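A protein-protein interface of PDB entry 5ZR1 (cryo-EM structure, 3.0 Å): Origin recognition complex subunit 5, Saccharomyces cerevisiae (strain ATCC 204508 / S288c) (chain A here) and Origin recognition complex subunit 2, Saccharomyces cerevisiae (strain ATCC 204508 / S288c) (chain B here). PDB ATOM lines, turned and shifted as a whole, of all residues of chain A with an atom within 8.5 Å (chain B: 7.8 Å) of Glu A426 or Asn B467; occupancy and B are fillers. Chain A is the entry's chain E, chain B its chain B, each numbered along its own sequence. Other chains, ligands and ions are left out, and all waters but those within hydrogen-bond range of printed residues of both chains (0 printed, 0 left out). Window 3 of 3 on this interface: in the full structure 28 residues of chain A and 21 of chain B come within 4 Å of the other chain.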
ATOM      1  N   LEU A 324      -8.304  -8.673 -11.904  1.00  0.00           N
ATOM      2  CA  LEU A 324      -9.540  -9.424 -12.019  1.00  0.00           C
ATOM      3  C   LEU A 324      -9.887  -9.686 -13.479  1.00  0.00           C
ATOM      4  O   LEU A 324      -9.357  -9.061 -14.401  1.00  0.00           O
ATOM      5  CB  LEU A 324     -10.689  -8.675 -11.352  1.00  0.00           C
ATOM      6  CG  LEU A 324     -10.590  -8.505  -9.841  1.00  0.00           C
ATOM      7  CD1 LEU A 324     -11.721  -7.639  -9.344  1.00  0.00           C
ATOM      8  CD2 LEU A 324     -10.565  -9.845  -9.135  1.00  0.00           C
ATOM      9  N   SER A 325     -10.804 -10.629 -13.672  1.00  0.00           N
ATOM     10  CA  SER A 325     -11.346 -10.936 -14.981  1.00  0.00           C
ATOM     11  C   SER A 325     -12.148  -9.764 -15.530  1.00  0.00           C
ATOM     12  O   SER A 325     -12.527  -8.849 -14.804  1.00  0.00           O
ATOM     13  CB  SER A 325     -12.237 -12.165 -14.902  1.00  0.00           C
ATOM     14  OG  SER A 325     -12.953 -12.314 -16.105  1.00  0.00           O
ATOM     15  N   SER A 328     -15.461 -10.178 -13.927  1.00  0.00           N
ATOM     16  CA  SER A 328     -15.355  -9.879 -12.504  1.00  0.00           C
ATOM     17  C   SER A 328     -15.257  -8.385 -12.275  1.00  0.00           C
ATOM     18  O   SER A 328     -15.637  -7.888 -11.212  1.00  0.00           O
ATOM     19  CB  SER A 328     -14.124 -10.550 -11.901  1.00  0.00           C
ATOM     20  OG  SER A 328     -14.181 -11.954 -11.998  1.00  0.00           O
ATOM     21  N   LEU A 331     -18.610  -6.856 -12.445  1.00  0.00           N
ATOM     22  CA  LEU A 331     -19.505  -7.415 -11.447  1.00  0.00           C
ATOM     23  C   LEU A 331     -19.254  -6.829 -10.067  1.00  0.00           C
ATOM     24  O   LEU A 331     -20.092  -6.997  -9.178  1.00  0.00           O
ATOM     25  CB  LEU A 331     -19.363  -8.941 -11.435  1.00  0.00           C
ATOM     26  CG  LEU A 331     -20.278  -9.960 -10.771  1.00  0.00           C
ATOM     27  CD1 LEU A 331     -21.682  -9.874 -11.318  1.00  0.00           C
ATOM     28  CD2 LEU A 331     -19.708 -11.320 -11.078  1.00  0.00           C
ATOM     29  N   ILE A 418     -21.864 -20.287 -16.575  1.00  0.00           N
ATOM     30  CA  ILE A 418     -21.206 -20.882 -15.417  1.00  0.00           C
ATOM     31  C   ILE A 418     -20.088 -19.986 -14.891  1.00  0.00           C
ATOM     32  O   ILE A 418     -19.688 -20.121 -13.732  1.00  0.00           O
ATOM     33  CB  ILE A 418     -20.666 -22.286 -15.777  1.00  0.00           C
ATOM     34  CG1 ILE A 418     -20.743 -23.226 -14.592  1.00  0.00           C
ATOM     35  CG2 ILE A 418     -19.214 -22.271 -16.244  1.00  0.00           C
ATOM     36  CD1 ILE A 418     -22.108 -23.756 -14.418  1.00  0.00           C
ATOM     37  N   GLU A 419     -19.594 -19.053 -15.712  1.00  0.00           N
ATOM     38  CA  GLU A 419     -18.469 -18.207 -15.342  1.00  0.00           C
ATOM     39  C   GLU A 419     -18.897 -16.989 -14.545  1.00  0.00           C
ATOM     40  O   GLU A 419     -18.102 -16.469 -13.759  1.00  0.00           O
ATOM     41  CB  GLU A 419     -17.733 -17.747 -16.593  1.00  0.00           C
ATOM     42  CG  GLU A 419     -16.923 -18.808 -17.280  1.00  0.00           C
ATOM     43  CD  GLU A 419     -16.336 -18.309 -18.575  1.00  0.00           C
ATOM     44  OE1 GLU A 419     -16.796 -17.262 -19.071  1.00  0.00           O
ATOM     45  OE2 GLU A 419     -15.383 -18.938 -19.075  1.00  0.00           O
ATOM     46  N   VAL A 420     -20.119 -16.504 -14.764  1.00  0.00           N
ATOM     47  CA  VAL A 420     -20.619 -15.361 -14.009  1.00  0.00           C
ATOM     48  C   VAL A 420     -20.793 -15.732 -12.543  1.00  0.00           C
ATOM     49  O   VAL A 420     -20.425 -14.965 -11.648  1.00  0.00           O
ATOM     50  CB  VAL A 420     -21.931 -14.855 -14.635  1.00  0.00           C
ATOM     51  CG1 VAL A 420     -22.509 -13.708 -13.834  1.00  0.00           C
ATOM     52  CG2 VAL A 420     -21.695 -14.432 -16.064  1.00  0.00           C
ATOM     53  N   PHE A 421     -21.315 -16.928 -12.275  1.00  0.00           N
ATOM     54  CA  PHE A 421     -21.446 -17.400 -10.903  1.00  0.00           C
ATOM     55  C   PHE A 421     -20.119 -17.846 -10.311  1.00  0.00           C
ATOM     56  O   PHE A 421     -19.932 -17.753  -9.096  1.00  0.00           O
ATOM     57  CB  PHE A 421     -22.442 -18.547 -10.835  1.00  0.00           C
ATOM     58  CG  PHE A 421     -23.856 -18.124 -11.023  1.00  0.00           C
ATOM     59  CD1 PHE A 421     -24.551 -17.539  -9.982  1.00  0.00           C
ATOM     60  CD2 PHE A 421     -24.497 -18.317 -12.230  1.00  0.00           C
ATOM     61  CE1 PHE A 421     -25.853 -17.146 -10.142  1.00  0.00           C
ATOM     62  CE2 PHE A 421     -25.804 -17.927 -12.395  1.00  0.00           C
ATOM     63  CZ  PHE A 421     -26.482 -17.340 -11.350  1.00  0.00           C
ATOM     64  N   GLN A 422     -19.207 -18.353 -11.139  1.00  0.00           N
ATOM     65  CA  GLN A 422     -17.891 -18.731 -10.641  1.00  0.00           C
ATOM     66  C   GLN A 422     -17.072 -17.502 -10.278  1.00  0.00           C
ATOM     67  O   GLN A 422     -16.321 -17.512  -9.297  1.00  0.00           O
ATOM     68  CB  GLN A 422     -17.160 -19.570 -11.685  1.00  0.00           C
ATOM     69  CG  GLN A 422     -15.829 -20.098 -11.224  1.00  0.00           C
ATOM     70  CD  GLN A 422     -15.110 -20.867 -12.296  1.00  0.00           C
ATOM     71  OE1 GLN A 422     -15.603 -21.006 -13.411  1.00  0.00           O
ATOM     72  NE2 GLN A 422     -13.925 -21.357 -11.974  1.00  0.00           N
ATOM     73  N   ASN A 423     -17.222 -16.424 -11.044  1.00  0.00           N
ATOM     74  CA  ASN A 423     -16.526 -15.186 -10.735  1.00  0.00           C
ATOM     75  C   ASN A 423     -17.212 -14.384  -9.645  1.00  0.00           C
ATOM     76  O   ASN A 423     -16.556 -13.562  -9.006  1.00  0.00           O
ATOM     77  CB  ASN A 423     -16.388 -14.333 -11.991  1.00  0.00           C
ATOM     78  CG  ASN A 423     -15.370 -14.892 -12.954  1.00  0.00           C
ATOM     79  OD1 ASN A 423     -14.277 -15.290 -12.559  1.00  0.00           O
ATOM     80  ND2 ASN A 423     -15.730 -14.957 -14.219  1.00  0.00           N
ATOM     81  N   LEU A 424     -18.506 -14.593  -9.424  1.00  0.00           N
ATOM     82  CA  LEU A 424     -19.170 -13.932  -8.311  1.00  0.00           C
ATOM     83  C   LEU A 424     -18.812 -14.611  -7.001  1.00  0.00           C
ATOM     84  O   LEU A 424     -18.730 -13.951  -5.963  1.00  0.00           O
ATOM     85  CB  LEU A 424     -20.682 -13.952  -8.522  1.00  0.00           C
ATOM     86  CG  LEU A 424     -21.615 -12.919  -7.888  1.00  0.00           C
ATOM     87  CD1 LEU A 424     -22.888 -12.923  -8.698  1.00  0.00           C
ATOM     88  CD2 LEU A 424     -21.923 -13.116  -6.413  1.00  0.00           C
ATOM     89  N   SER A 425     -18.601 -15.924  -7.037  1.00  0.00           N
ATOM     90  CA  SER A 425     -18.181 -16.659  -5.855  1.00  0.00           C
ATOM     91  C   SER A 425     -16.712 -16.432  -5.541  1.00  0.00           C
ATOM     92  O   SER A 425     -16.332 -16.424  -4.368  1.00  0.00           O
ATOM     93  CB  SER A 425     -18.447 -18.147  -6.052  1.00  0.00           C
ATOM     94  OG  SER A 425     -18.010 -18.884  -4.930  1.00  0.00           O
ATOM     95  N   GLU A 426     -15.876 -16.262  -6.566  1.00  0.00           N
ATOM     96  CA  GLU A 426     -14.477 -15.903  -6.353  1.00  0.00           C
ATOM     97  C   GLU A 426     -14.351 -14.491  -5.814  1.00  0.00           C
ATOM     98  O   GLU A 426     -13.440 -14.199  -5.035  1.00  0.00           O
ATOM     99  CB  GLU A 426     -13.707 -16.042  -7.666  1.00  0.00           C
ATOM    100  CG  GLU A 426     -12.215 -15.728  -7.622  1.00  0.00           C
ATOM    101  CD  GLU A 426     -11.399 -16.756  -6.851  1.00  0.00           C
ATOM    102  OE1 GLU A 426     -11.883 -17.887  -6.648  1.00  0.00           O
ATOM    103  OE2 GLU A 426     -10.242 -16.451  -6.497  1.00  0.00           O
ATOM    104  N   LEU A 427     -15.275 -13.615  -6.194  1.00  0.00           N
ATOM    105  CA  LEU A 427     -15.269 -12.241  -5.722  1.00  0.00           C
ATOM    106  C   LEU A 427     -15.696 -12.157  -4.264  1.00  0.00           C
ATOM    107  O   LEU A 427     -15.383 -11.175  -3.589  1.00  0.00           O
ATOM    108  CB  LEU A 427     -16.197 -11.426  -6.614  1.00  0.00           C
ATOM    109  CG  LEU A 427     -16.111  -9.928  -6.805  1.00  0.00           C
ATOM    110  CD1 LEU A 427     -14.810  -9.638  -7.502  1.00  0.00           C
ATOM    111  CD2 LEU A 427     -17.267  -9.505  -7.669  1.00  0.00           C
ATOM    112  N   HIS A 428     -16.391 -13.182  -3.772  1.00  0.00           N
ATOM    113  CA  HIS A 428     -16.792 -13.275  -2.377  1.00  0.00           C
ATOM    114  C   HIS A 428     -15.704 -13.864  -1.494  1.00  0.00           C
ATOM    115  O   HIS A 428     -15.574 -13.463  -0.332  1.00  0.00           O
ATOM    116  CB  HIS A 428     -18.069 -14.104  -2.268  1.00  0.00           C
ATOM    117  CG  HIS A 428     -18.499 -14.378  -0.864  1.00  0.00           C
ATOM    118  ND1 HIS A 428     -18.189 -15.551  -0.213  1.00  0.00           N
ATOM    119  CD2 HIS A 428     -19.169 -13.617   0.030  1.00  0.00           C
ATOM    120  CE1 HIS A 428     -18.682 -15.515   1.011  1.00  0.00           C
ATOM    121  NE2 HIS A 428     -19.278 -14.350   1.186  1.00  0.00           N
ATOM    122  N   THR A 429     -14.911 -14.803  -2.012  1.00  0.00           N
ATOM    123  CA  THR A 429     -13.824 -15.367  -1.223  1.00  0.00           C
ATOM    124  C   THR A 429     -12.664 -14.400  -1.082  1.00  0.00           C
ATOM    125  O   THR A 429     -11.857 -14.545  -0.160  1.00  0.00           O
ATOM    126  CB  THR A 429     -13.326 -16.667  -1.850  1.00  0.00           C
ATOM    127  OG1 THR A 429     -12.822 -16.402  -3.162  1.00  0.00           O
ATOM    128  CG2 THR A 429     -14.454 -17.675  -1.933  1.00  0.00           C
ATOM    129  N   LEU A 430     -12.573 -13.420  -1.971  1.00  0.00           N
ATOM    130  CA  LEU A 430     -11.556 -12.382  -1.950  1.00  0.00           C
ATOM    131  C   LEU A 430     -11.963 -11.196  -1.096  1.00  0.00           C
ATOM    132  O   LEU A 430     -11.240 -10.194  -1.075  1.00  0.00           O
ATOM    133  CB  LEU A 430     -11.265 -11.933  -3.383  1.00  0.00           C
ATOM    134  CG  LEU A 430     -10.161 -12.605  -4.197  1.00  0.00           C
ATOM    135  CD1 LEU A 430     -10.259 -14.103  -4.233  1.00  0.00           C
ATOM    136  CD2 LEU A 430     -10.283 -12.087  -5.618  1.00  0.00           C
ATOM    137  N   LYS A 431     -13.110 -11.303  -0.413  1.00  0.00           N
ATOM    138  CA  LYS A 431     -13.670 -10.281   0.478  1.00  0.00           C
ATOM    139  C   LYS A 431     -13.917  -8.966  -0.258  1.00  0.00           C
ATOM    140  O   LYS A 431     -13.719  -7.881   0.287  1.00  0.00           O
ATOM    141  CB  LYS A 431     -12.790 -10.070   1.712  1.00  0.00           C
ATOM    142  CG  LYS A 431     -12.535 -11.344   2.496  1.00  0.00           C
ATOM    143  CD  LYS A 431     -13.808 -11.887   3.113  1.00  0.00           C
ATOM    144  CE  LYS A 431     -13.522 -13.104   3.975  1.00  0.00           C
ATOM    145  NZ  LYS A 431     -13.141 -14.285   3.153  1.00  0.00           N
ATOM    146  N   LEU A 432     -14.353  -9.068  -1.515  1.00  0.00           N
ATOM    147  CA  LEU A 432     -14.775  -7.905  -2.280  1.00  0.00           C
ATOM    148  C   LEU A 432     -16.289  -7.773  -2.341  1.00  0.00           C
ATOM    149  O   LEU A 432     -16.788  -6.674  -2.595  1.00  0.00           O
ATOM    150  CB  LEU A 432     -14.208  -7.960  -3.702  1.00  0.00           C
ATOM    151  CG  LEU A 432     -12.681  -8.010  -3.821  1.00  0.00           C
ATOM    152  CD1 LEU A 432     -12.250  -8.033  -5.273  1.00  0.00           C
ATOM    153  CD2 LEU A 432     -12.005  -6.882  -3.075  1.00  0.00           C
ATOM    154  N   ILE A 433     -17.019  -8.862  -2.118  1.00  0.00           N
ATOM    155  CA  ILE A 433     -18.455  -8.847  -1.870  1.00  0.00           C
ATOM    156  C   ILE A 433     -18.671  -9.403  -0.472  1.00  0.00           C
ATOM    157  O   ILE A 433     -18.068 -10.415  -0.103  1.00  0.00           O
ATOM    158  CB  ILE A 433     -19.232  -9.683  -2.907  1.00  0.00           C
ATOM    159  CG1 ILE A 433     -18.851  -9.279  -4.321  1.00  0.00           C
ATOM    160  CG2 ILE A 433     -20.709  -9.465  -2.766  1.00  0.00           C
ATOM    161  CD1 ILE A 433     -19.150  -7.863  -4.638  1.00  0.00           C
ATOM    162  N   TYR A 443     -25.067 -19.739   0.506  1.00  0.00           N
ATOM    163  CA  TYR A 443     -25.258 -18.959  -0.712  1.00  0.00           C
ATOM    164  C   TYR A 443     -26.638 -19.191  -1.304  1.00  0.00           C
ATOM    165  O   TYR A 443     -27.234 -18.280  -1.887  1.00  0.00           O
ATOM    166  CB  TYR A 443     -24.218 -19.373  -1.751  1.00  0.00           C
ATOM    167  CG  TYR A 443     -22.770 -19.203  -1.369  1.00  0.00           C
ATOM    168  CD1 TYR A 443     -22.098 -18.017  -1.617  1.00  0.00           C
ATOM    169  CD2 TYR A 443     -22.071 -20.239  -0.770  1.00  0.00           C
ATOM    170  CE1 TYR A 443     -20.764 -17.866  -1.279  1.00  0.00           C
ATOM    171  CE2 TYR A 443     -20.742 -20.099  -0.424  1.00  0.00           C
ATOM    172  CZ  TYR A 443     -20.094 -18.913  -0.681  1.00  0.00           C
ATOM    173  OH  TYR A 443     -18.772 -18.779  -0.335  1.00  0.00           O
ATOM    174  N   TRP A 450     -26.492  -9.469  -0.071  1.00  0.00           N
ATOM    175  CA  TRP A 450     -25.123  -9.237  -0.479  1.00  0.00           C
ATOM    176  C   TRP A 450     -24.854  -7.744  -0.455  1.00  0.00           C
ATOM    177  O   TRP A 450     -25.765  -6.930  -0.589  1.00  0.00           O
ATOM    178  CB  TRP A 450     -24.901  -9.797  -1.883  1.00  0.00           C
ATOM    179  CG  TRP A 450     -25.096 -11.270  -1.960  1.00  0.00           C
ATOM    180  CD1 TRP A 450     -26.276 -11.929  -2.124  1.00  0.00           C
ATOM    181  CD2 TRP A 450     -24.080 -12.272  -1.938  1.00  0.00           C
ATOM    182  NE1 TRP A 450     -26.060 -13.283  -2.161  1.00  0.00           N
ATOM    183  CE2 TRP A 450     -24.718 -13.517  -2.055  1.00  0.00           C
ATOM    184  CE3 TRP A 450     -22.693 -12.237  -1.814  1.00  0.00           C
ATOM    185  CZ2 TRP A 450     -24.015 -14.712  -2.056  1.00  0.00           C
ATOM    186  CZ3 TRP A 450     -22.003 -13.416  -1.818  1.00  0.00           C
ATOM    187  CH2 TRP A 450     -22.659 -14.638  -1.938  1.00  0.00           C
ATOM    188  N   PRO B 462     -24.321 -22.939  -9.331  1.00  0.00           N
ATOM    189  CA  PRO B 462     -22.921 -22.608  -9.650  1.00  0.00           C
ATOM    190  C   PRO B 462     -22.333 -21.473  -8.832  1.00  0.00           C
ATOM    191  O   PRO B 462     -21.128 -21.223  -8.947  1.00  0.00           O
ATOM    192  CB  PRO B 462     -22.979 -22.226 -11.129  1.00  0.00           C
ATOM    193  CG  PRO B 462     -24.179 -22.825 -11.618  1.00  0.00           C
ATOM    194  CD  PRO B 462     -25.142 -22.747 -10.542  1.00  0.00           C
ATOM    195  N   LEU B 463     -23.129 -20.788  -8.008  1.00  0.00           N
ATOM    196  CA  LEU B 463     -22.636 -19.781  -7.076  1.00  0.00           C
ATOM    197  C   LEU B 463     -21.870 -20.403  -5.919  1.00  0.00           C
ATOM    198  O   LEU B 463     -21.209 -19.692  -5.158  1.00  0.00           O
ATOM    199  CB  LEU B 463     -23.824 -18.964  -6.558  1.00  0.00           C
ATOM    200  CG  LEU B 463     -23.692 -17.702  -5.713  1.00  0.00           C
ATOM    201  CD1 LEU B 463     -22.989 -16.654  -6.523  1.00  0.00           C
ATOM    202  CD2 LEU B 463     -25.048 -17.210  -5.262  1.00  0.00           C
ATOM    203  N   TRP B 465     -19.372 -22.655  -6.040  1.00  0.00           N
ATOM    204  CA  TRP B 465     -17.992 -23.051  -6.304  1.00  0.00           C
ATOM    205  C   TRP B 465     -17.245 -21.869  -6.902  1.00  0.00           C
ATOM    206  O   TRP B 465     -17.622 -21.371  -7.967  1.00  0.00           O
ATOM    207  CB  TRP B 465     -17.919 -24.245  -7.260  1.00  0.00           C
ATOM    208  CG  TRP B 465     -18.949 -25.287  -7.000  1.00  0.00           C
ATOM    209  CD1 TRP B 465     -19.051 -26.097  -5.915  1.00  0.00           C
ATOM    210  CD2 TRP B 465     -19.969 -25.701  -7.906  1.00  0.00           C
ATOM    211  NE1 TRP B 465     -20.122 -26.946  -6.063  1.00  0.00           N
ATOM    212  CE2 TRP B 465     -20.692 -26.725  -7.284  1.00  0.00           C
ATOM    213  CE3 TRP B 465     -20.360 -25.279  -9.181  1.00  0.00           C
ATOM    214  CZ2 TRP B 465     -21.774 -27.338  -7.886  1.00  0.00           C
ATOM    215  CZ3 TRP B 465     -21.426 -25.893  -9.778  1.00  0.00           C
ATOM    216  CH2 TRP B 465     -22.127 -26.907  -9.130  1.00  0.00           C
ATOM    217  N   ASP B 466     -16.176 -21.441  -6.233  1.00  0.00           N
ATOM    218  CA  ASP B 466     -15.284 -20.401  -6.735  1.00  0.00           C
ATOM    219  C   ASP B 466     -14.258 -20.978  -7.704  1.00  0.00           C
ATOM    220  O   ASP B 466     -14.427 -22.105  -8.171  1.00  0.00           O
ATOM    221  CB  ASP B 466     -14.589 -19.683  -5.577  1.00  0.00           C
ATOM    222  CG  ASP B 466     -13.860 -20.631  -4.648  1.00  0.00           C
ATOM    223  OD1 ASP B 466     -14.003 -21.859  -4.792  1.00  0.00           O
ATOM    224  OD2 ASP B 466     -13.127 -20.147  -3.765  1.00  0.00           O
ATOM    225  N   ASN B 467     -13.195 -20.226  -8.013  1.00  0.00           N
ATOM    226  CA  ASN B 467     -12.195 -20.727  -8.952  1.00  0.00           C
ATOM    227  C   ASN B 467     -11.384 -21.882  -8.382  1.00  0.00           C
ATOM    228  O   ASN B 467     -10.940 -22.748  -9.142  1.00  0.00           O
ATOM    229  CB  ASN B 467     -11.242 -19.617  -9.399  1.00  0.00           C
ATOM    230  CG  ASN B 467     -11.866 -18.679 -10.401  1.00  0.00           C
ATOM    231  OD1 ASN B 467     -12.686 -19.087 -11.217  1.00  0.00           O
ATOM    232  ND2 ASN B 467     -11.436 -17.429 -10.388  1.00  0.00           N
ATOM    233  N   MET B 468     -11.169 -21.921  -7.069  1.00  0.00           N
ATOM    234  CA  MET B 468     -10.382 -23.016  -6.513  1.00  0.00           C
ATOM    235  C   MET B 468     -11.195 -24.301  -6.444  1.00  0.00           C
ATOM    236  O   MET B 468     -10.678 -25.376  -6.757  1.00  0.00           O
ATOM    237  CB  MET B 468      -9.849 -22.652  -5.130  1.00  0.00           C
ATOM    238  CG  MET B 468      -8.790 -23.616  -4.618  1.00  0.00           C
ATOM    239  SD  MET B 468      -7.284 -23.503  -5.606  1.00  0.00           S
ATOM    240  CE  MET B 468      -6.554 -25.111  -5.322  1.00  0.00           C
ATOM    241  N   LYS B 469     -12.470 -24.209  -6.062  1.00  0.00           N
ATOM    242  CA  LYS B 469     -13.300 -25.404  -5.988  1.00  0.00           C
ATOM    243  C   LYS B 469     -13.701 -25.914  -7.361  1.00  0.00           C
ATOM    244  O   LYS B 469     -13.886 -27.120  -7.534  1.00  0.00           O
ATOM    245  CB  LYS B 469     -14.545 -25.141  -5.152  1.00  0.00           C
ATOM    246  CG  LYS B 469     -14.264 -25.032  -3.681  1.00  0.00           C
ATOM    247  CD  LYS B 469     -15.537 -24.852  -2.906  1.00  0.00           C
ATOM    248  CE  LYS B 469     -15.237 -24.728  -1.434  1.00  0.00           C
ATOM    249  NZ  LYS B 469     -16.469 -24.472  -0.655  1.00  0.00           N
ATOM    250  N   ALA B 470     -13.853 -25.030  -8.345  1.00  0.00           N
ATOM    251  CA  ALA B 470     -14.160 -25.501  -9.688  1.00  0.00           C
ATOM    252  C   ALA B 470     -12.949 -26.121 -10.364  1.00  0.00           C
ATOM    253  O   ALA B 470     -13.113 -26.910 -11.296  1.00  0.00           O
ATOM    254  CB  ALA B 470     -14.702 -24.363 -10.545  1.00  0.00           C
ATOM    255  N   GLN B 471     -11.743 -25.767  -9.923  1.00  0.00           N
ATOM    256  CA  GLN B 471     -10.541 -26.424 -10.419  1.00  0.00           C
ATOM    257  C   GLN B 471     -10.433 -27.845  -9.890  1.00  0.00           C
ATOM    258  O   GLN B 471     -10.152 -28.781 -10.648  1.00  0.00           O
ATOM    259  CB  GLN B 471      -9.307 -25.628 -10.016  1.00  0.00           C
ATOM    260  CG  GLN B 471      -8.020 -26.273 -10.450  1.00  0.00           C
ATOM    261  CD  GLN B 471      -6.806 -25.544  -9.943  1.00  0.00           C
ATOM    262  OE1 GLN B 471      -6.920 -24.545  -9.238  1.00  0.00           O
ATOM    263  NE2 GLN B 471      -5.630 -26.049 -10.284  1.00  0.00           N
ATOM    264  N   ASN B 472     -10.637 -28.021  -8.581  1.00  0.00           N
ATOM    265  CA  ASN B 472     -10.507 -29.334  -7.962  1.00  0.00           C
ATOM    266  C   ASN B 472     -11.611 -30.276  -8.412  1.00  0.00           C
ATOM    267  O   ASN B 472     -11.382 -31.477  -8.584  1.00  0.00           O
ATOM    268  CB  ASN B 472     -10.515 -29.206  -6.442  1.00  0.00           C
ATOM    269  CG  ASN B 472      -9.326 -28.440  -5.911  1.00  0.00           C
ATOM    270  OD1 ASN B 472      -9.481 -27.459  -5.192  1.00  0.00           O
ATOM    271  ND2 ASN B 472      -8.132 -28.861  -6.291  1.00  0.00           N
ATOM    272  N   TYR B 473     -12.818 -29.748  -8.589  1.00  0.00           N
ATOM    273  CA  TYR B 473     -13.917 -30.530  -9.136  1.00  0.00           C
ATOM    274  C   TYR B 473     -13.685 -30.884 -10.599  1.00  0.00           C
ATOM    275  O   TYR B 473     -13.792 -32.052 -10.970  1.00  0.00           O
ATOM    276  CB  TYR B 473     -15.211 -29.748  -8.970  1.00  0.00           C
ATOM    277  CG  TYR B 473     -15.937 -29.938  -7.660  1.00  0.00           C
ATOM    278  CD1 TYR B 473     -15.959 -31.168  -7.020  1.00  0.00           C
ATOM    279  CD2 TYR B 473     -16.575 -28.870  -7.041  1.00  0.00           C
ATOM    280  CE1 TYR B 473     -16.646 -31.336  -5.830  1.00  0.00           C
ATOM    281  CE2 TYR B 473     -17.262 -29.033  -5.866  1.00  0.00           C
ATOM    282  CZ  TYR B 473     -17.283 -30.260  -5.258  1.00  0.00           C
ATOM    283  OH  TYR B 473     -17.960 -30.392  -4.072  1.00  0.00           O
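N of Asp B466 lies within hydrogen-bond range of OG of Ser A425 (3.4 Å). The side-chain carboxylate (OE1) of Glu A426 lies within hydrogen-bond range of the backbone NH (N) of Asn B467, at 3.0 Å. The side-chain amide nitrogen (NE2) of Gln A422 sits at hydrogen-bond distance from the side-chain amide oxygen (OD1) of Asn B467 (2.7 Å). The backbone carbonyl oxygen (O) of Leu B463 lies close to the side-chain hydroxyl (OG) of Ser A425 (3.3 Å).
The backbone NH (N) of Lys B469 is in hydrogen-bond range of the side-chain carboxylate (OD1) of Asp B466 (3.1 Å). OG1 of Thr A429 is in hydrogen-bond range of O of Glu A426, at 3.0 Å.
CD1 of Ile A418 touches CG of Pro B462, 3.6 Å away. O of Pro B462 touches CB of Phe A421, 3.5 Å away. Phe A421 touches Leu B463. Gln A422 touches Trp B465. Asp B466 touches Gln A422 (O to NE2, 3.9 Å). CB of Ala B470 touches NE2 of Gln A422 (3.4 Å). CD1 of Leu B463 touches CD2 of Leu A424, 3.7 Å away. Trp B465 touches Ser A425. CB of Asp B466 touches OE1 of Glu A426, at 3.4 Å. CG2 of Thr A429 touches OD2 of Asp B466 (3.4 Å).
Of chain A, only Gln A422 (2.7 Å) and Glu A426 (3.0 Å) come within 4 Å of Asn B467. Of chain A, only Gln A422, Ser A425, Glu A426 and Thr A429 come within 4 Å of Asp B466. Printed residues of chain B within 4 Å of Ile A418: Pro B462 (3.6 Å). Of the printed residues of chain A, Trp B465 touches Gln A422 and Ser A425. Of the printed residues of chain A, Ala B470 touches Gln A422 (3.4 Å). Leu A324 touches none of the printed residues of chain B. Asn B472 touches none of the printed residues of chain A.
Along chain A the printed residues that touch a printed residue of chain B span positions 418 to 429. Hydrophobic or aromatic side chains of chain B that line the printed part of chain A: Pro B462, Leu B463 and Ala B470. Among the printed residues, 14 pairs touch across the chains.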
